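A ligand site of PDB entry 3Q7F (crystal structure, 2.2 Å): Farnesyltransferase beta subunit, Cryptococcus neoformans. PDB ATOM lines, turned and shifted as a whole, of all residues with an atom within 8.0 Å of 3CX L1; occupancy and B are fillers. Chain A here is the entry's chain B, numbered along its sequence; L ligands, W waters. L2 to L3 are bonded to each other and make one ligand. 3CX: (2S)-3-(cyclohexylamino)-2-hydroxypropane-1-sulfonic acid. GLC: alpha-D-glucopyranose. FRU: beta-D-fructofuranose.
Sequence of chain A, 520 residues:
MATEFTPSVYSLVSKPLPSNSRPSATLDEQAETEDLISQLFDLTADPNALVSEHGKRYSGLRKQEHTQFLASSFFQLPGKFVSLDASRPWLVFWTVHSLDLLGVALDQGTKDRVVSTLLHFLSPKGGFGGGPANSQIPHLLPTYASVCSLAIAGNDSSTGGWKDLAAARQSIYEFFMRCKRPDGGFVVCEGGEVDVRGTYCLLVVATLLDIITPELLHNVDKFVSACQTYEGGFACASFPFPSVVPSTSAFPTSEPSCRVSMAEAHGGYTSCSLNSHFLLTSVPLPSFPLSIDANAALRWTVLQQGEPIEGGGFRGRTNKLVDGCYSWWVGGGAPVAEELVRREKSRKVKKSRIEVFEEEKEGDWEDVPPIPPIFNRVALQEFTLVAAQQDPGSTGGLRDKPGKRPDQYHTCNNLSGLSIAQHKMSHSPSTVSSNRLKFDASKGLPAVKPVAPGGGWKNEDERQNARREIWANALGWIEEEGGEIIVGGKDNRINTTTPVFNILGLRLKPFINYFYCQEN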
ATOM      1  N   TYR A  58      12.424 -14.515  -8.785  1.00  0.00           N
ATOM      2  CA  TYR A  58      12.556 -13.068  -8.831  1.00  0.00           C
ATOM      3  C   TYR A  58      13.033 -12.545  -7.474  1.00  0.00           C
ATOM      4  O   TYR A  58      12.497 -12.925  -6.430  1.00  0.00           O
ATOM      5  CB  TYR A  58      11.266 -12.385  -9.298  1.00  0.00           C
ATOM      6  CG  TYR A  58      11.387 -10.883  -9.399  1.00  0.00           C
ATOM      7  CD1 TYR A  58      10.543 -10.035  -8.686  1.00  0.00           C
ATOM      8  CD2 TYR A  58      12.379 -10.301 -10.197  1.00  0.00           C
ATOM      9  CE1 TYR A  58      10.663  -8.662  -8.767  1.00  0.00           C
ATOM     10  CE2 TYR A  58      12.502  -8.915 -10.291  1.00  0.00           C
ATOM     11  CZ  TYR A  58      11.650  -8.099  -9.569  1.00  0.00           C
ATOM     12  OH  TYR A  58      11.782  -6.738  -9.652  1.00  0.00           O
ATOM     13  N   GLY A  60      13.138  -9.296  -6.406  1.00  0.00           N
ATOM     14  CA  GLY A  60      12.550  -8.019  -5.983  1.00  0.00           C
ATOM     15  C   GLY A  60      12.228  -7.987  -4.492  1.00  0.00           C
ATOM     16  O   GLY A  60      11.819  -8.992  -3.917  1.00  0.00           O
ATOM     17  N   LEU A  61      12.421  -6.816  -3.884  1.00  0.00           N
ATOM     18  CA  LEU A  61      12.106  -6.645  -2.476  1.00  0.00           C
ATOM     19  C   LEU A  61      10.603  -6.804  -2.259  1.00  0.00           C
ATOM     20  O   LEU A  61       9.798  -6.056  -2.805  1.00  0.00           O
ATOM     21  CB  LEU A  61      12.594  -5.289  -1.956  1.00  0.00           C
ATOM     22  CG  LEU A  61      12.458  -5.021  -0.452  1.00  0.00           C
ATOM     23  CD1 LEU A  61      13.324  -5.961   0.384  1.00  0.00           C
ATOM     24  CD2 LEU A  61      12.794  -3.564  -0.122  1.00  0.00           C
ATOM     25  N   ILE A 486      20.337   1.863  -6.498  1.00  0.00           N
ATOM     26  CA  ILE A 486      19.257   0.946  -6.168  1.00  0.00           C
ATOM     27  C   ILE A 486      19.301  -0.279  -7.087  1.00  0.00           C
ATOM     28  O   ILE A 486      18.823  -0.245  -8.224  1.00  0.00           O
ATOM     29  CB  ILE A 486      17.846   1.609  -6.236  1.00  0.00           C
ATOM     30  CG1 ILE A 486      17.863   3.021  -5.629  1.00  0.00           C
ATOM     31  CG2 ILE A 486      16.791   0.712  -5.580  1.00  0.00           C
ATOM     32  CD1 ILE A 486      18.094   3.085  -4.123  1.00  0.00           C
ATOM     33  N   VAL A 487      19.909  -1.339  -6.575  1.00  0.00           N
ATOM     34  CA  VAL A 487      20.060  -2.605  -7.292  1.00  0.00           C
ATOM     35  C   VAL A 487      18.686  -3.219  -7.563  1.00  0.00           C
ATOM     36  O   VAL A 487      17.866  -3.362  -6.651  1.00  0.00           O
ATOM     37  CB  VAL A 487      20.958  -3.584  -6.506  1.00  0.00           C
ATOM     38  CG1 VAL A 487      20.927  -4.993  -7.113  1.00  0.00           C
ATOM     39  CG2 VAL A 487      22.390  -3.063  -6.438  1.00  0.00           C
ATOM     40  N   GLY A 488      18.429  -3.560  -8.831  1.00  0.00           N
ATOM     41  CA  GLY A 488      17.182  -4.203  -9.228  1.00  0.00           C
ATOM     42  C   GLY A 488      16.086  -3.230  -9.650  1.00  0.00           C
ATOM     43  O   GLY A 488      14.986  -3.651 -10.030  1.00  0.00           O
ATOM     44  N   GLY A 489      16.366  -1.941  -9.588  1.00  0.00           N
ATOM     45  CA  GLY A 489      15.402  -0.927 -10.009  1.00  0.00           C
ATOM     46  C   GLY A 489      14.758  -0.195  -8.849  1.00  0.00           C
ATOM     47  O   GLY A 489      14.850  -0.640  -7.699  1.00  0.00           O
ATOM     48  N   LYS A 490      14.081   0.907  -9.153  1.00  0.00           N
ATOM     49  CA  LYS A 490      13.596   1.846  -8.142  1.00  0.00           C
ATOM     50  C   LYS A 490      12.500   1.328  -7.211  1.00  0.00           C
ATOM     51  O   LYS A 490      12.310   1.871  -6.132  1.00  0.00           O
ATOM     52  CB  LYS A 490      13.197   3.172  -8.786  1.00  0.00           C
ATOM     53  CG  LYS A 490      14.386   3.913  -9.391  1.00  0.00           C
ATOM     54  CD  LYS A 490      13.985   5.226 -10.023  1.00  0.00           C
ATOM     55  CE  LYS A 490      15.188   5.932 -10.627  1.00  0.00           C
ATOM     56  NZ  LYS A 490      14.817   7.266 -11.176  1.00  0.00           N
ATOM     57  N   ASP A 491      11.799   0.285  -7.620  1.00  0.00           N
ATOM     58  CA  ASP A 491      10.804  -0.353  -6.738  1.00  0.00           C
ATOM     59  C   ASP A 491      11.449  -1.025  -5.518  1.00  0.00           C
ATOM     60  O   ASP A 491      10.777  -1.261  -4.514  1.00  0.00           O
ATOM     61  CB  ASP A 491       9.942  -1.345  -7.511  1.00  0.00           C
ATOM     62  CG  ASP A 491       8.948  -0.661  -8.443  1.00  0.00           C
ATOM     63  OD1 ASP A 491       8.274   0.314  -8.030  1.00  0.00           O
ATOM     64  OD2 ASP A 491       8.814  -1.116  -9.586  1.00  0.00           O
ATOM     65  N   ASN A 492      12.743  -1.319  -5.608  1.00  0.00           N
ATOM     66  CA  ASN A 492      13.500  -1.840  -4.454  1.00  0.00           C
ATOM     67  C   ASN A 492      13.944  -0.778  -3.447  1.00  0.00           C
ATOM     68  O   ASN A 492      14.421  -1.115  -2.363  1.00  0.00           O
ATOM     69  CB  ASN A 492      14.724  -2.624  -4.918  1.00  0.00           C
ATOM     70  CG  ASN A 492      14.363  -3.954  -5.527  1.00  0.00           C
ATOM     71  OD1 ASN A 492      13.261  -4.475  -5.335  1.00  0.00           O
ATOM     72  ND2 ASN A 492      15.299  -4.525  -6.277  1.00  0.00           N
ATOM     73  N   ARG A 493      13.778   0.502  -3.797  1.00  0.00           N
ATOM     74  CA  ARG A 493      14.214   1.613  -2.940  1.00  0.00           C
ATOM     75  C   ARG A 493      13.482   1.657  -1.606  1.00  0.00           C
ATOM     76  O   ARG A 493      12.254   1.648  -1.548  1.00  0.00           O
ATOM     77  CB  ARG A 493      14.036   2.960  -3.651  1.00  0.00           C
ATOM     78  CG  ARG A 493      14.584   4.160  -2.856  1.00  0.00           C
ATOM     79  CD  ARG A 493      13.930   5.475  -3.274  1.00  0.00           C
ATOM     80  NE  ARG A 493      14.477   6.609  -2.519  1.00  0.00           N
ATOM     81  CZ  ARG A 493      14.013   7.022  -1.336  1.00  0.00           C
ATOM     82  NH1 ARG A 493      12.985   6.413  -0.750  1.00  0.00           N
ATOM     83  NH2 ARG A 493      14.576   8.063  -0.727  1.00  0.00           N
HETATM   84  OAA 3CX L   1      13.371   2.328 -14.104  1.00  0.00           O
HETATM   85  OAB 3CX L   1      12.214   2.745 -12.060  1.00  0.00           O
HETATM   86  OAC 3CX L   1      11.118   0.166 -10.924  1.00  0.00           O
HETATM   87  OAD 3CX L   1      14.140   1.315 -12.068  1.00  0.00           O
HETATM   88  CAE 3CX L   1       7.112  -5.413 -11.476  1.00  0.00           C
HETATM   89  CAF 3CX L   1       7.303  -4.528 -12.669  1.00  0.00           C
HETATM   90  CAG 3CX L   1       8.417  -5.777 -10.831  1.00  0.00           C
HETATM   91  CAH 3CX L   1       8.144  -3.332 -12.369  1.00  0.00           C
HETATM   92  CAI 3CX L   1       9.261  -4.574 -10.516  1.00  0.00           C
HETATM   93  CAJ 3CX L   1      10.753  -1.749 -12.282  1.00  0.00           C
HETATM   94  CAK 3CX L   1      11.927   0.343 -13.137  1.00  0.00           C
HETATM   95  NAL 3CX L   1      10.111  -2.463 -11.211  1.00  0.00           N
HETATM   96  CAM 3CX L   1      11.333  -0.396 -11.991  1.00  0.00           C
HETATM   97  CAN 3CX L   1       9.442  -3.669 -11.691  1.00  0.00           C
HETATM   98  SAO 3CX L   1      12.955   1.742 -12.823  1.00  0.00           S
HETATM   99  C1  GLC L   2      19.714   0.315 -12.595  1.00  0.00           C
HETATM  100  C2  GLC L   2      19.040  -1.005 -12.895  1.00  0.00           C
HETATM  101  C3  GLC L   2      19.969  -2.196 -12.900  1.00  0.00           C
HETATM  102  C4  GLC L   2      20.905  -2.232 -11.725  1.00  0.00           C
HETATM  103  C5  GLC L   2      21.082  -0.838 -11.170  1.00  0.00           C
HETATM  104  C6  GLC L   2      22.344  -0.726 -10.385  1.00  0.00           C
HETATM  105  O2  GLC L   2      18.409  -0.902 -14.100  1.00  0.00           O
HETATM  106  O3  GLC L   2      19.186  -3.333 -12.966  1.00  0.00           O
HETATM  107  O4  GLC L   2      20.522  -3.130 -10.729  1.00  0.00           O
HETATM  108  O5  GLC L   2      21.038   0.159 -12.151  1.00  0.00           O
HETATM  109  O6  GLC L   2      23.471  -0.907 -11.181  1.00  0.00           O
HETATM  110  C1  FRU L   3      17.642   2.567 -12.853  1.00  0.00           C
HETATM  111  C2  FRU L   3      18.701   2.362 -11.830  1.00  0.00           C
HETATM  112  C3  FRU L   3      18.306   2.919 -10.491  1.00  0.00           C
HETATM  113  C4  FRU L   3      19.506   3.626  -9.975  1.00  0.00           C
HETATM  114  C5  FRU L   3      20.561   3.320 -10.972  1.00  0.00           C
HETATM  115  C6  FRU L   3      21.574   4.417 -11.113  1.00  0.00           C
HETATM  116  O1  FRU L   3      17.152   3.860 -12.836  1.00  0.00           O
HETATM  117  O2  FRU L   3      18.922   0.970 -11.629  1.00  0.00           O
HETATM  118  O3  FRU L   3      17.825   1.934  -9.640  1.00  0.00           O
HETATM  119  O4  FRU L   3      19.885   3.209  -8.718  1.00  0.00           O
HETATM  120  O5  FRU L   3      19.886   3.018 -12.184  1.00  0.00           O
HETATM  121  O6  FRU L   3      22.823   3.817 -11.063  1.00  0.00           O
HETATM  122  O   HOH W   1      15.491  -0.782 -13.422  1.00  0.00           O
HETATM  123  O   HOH W   2      12.591   1.510 -16.857  1.00  0.00           O
HETATM  124  O   HOH W   3      12.501  -2.781  -9.405  1.00  0.00           O
HETATM  125  O   HOH W   4      12.898  -4.243 -12.468  1.00  0.00           O
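Water W1 bridges an oxygen (OAD) of 3CX L1 (2.8 Å) and an oxygen (O2) of GLC L2 (3.0 Å). Water W3 lies within hydrogen-bond range of the backbone carbonyl oxygen of Gly 488 and a nitrogen (NAL) of 3CX L1.
OH of Tyr 58 touches CAI of 3CX L1, 3.4 Å away. Gly 489 touches 3CX L1.
N of Asp 491 sits at hydrogen-bond distance from OAC of 3CX L1 (3.4 Å). OD2 of Asp 491 lies within salt-bridge range of NAL of 3CX L1, at 2.5 Å. An oxygen (OAD) of 3CX L1 sits at hydrogen-bond distance from the backbone NH (N) of Lys 490, 2.9 Å away. O4 of GLC L2 sits at hydrogen-bond distance from N of Gly 488, at 2.9 Å. The backbone NH (N) of Ile 486 lies within hydrogen-bond range of an oxygen (O4) of FRU L3 (2.6 Å). O3 of FRU L3 lies within hydrogen-bond range of O of Ile 486 (2.8 Å).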
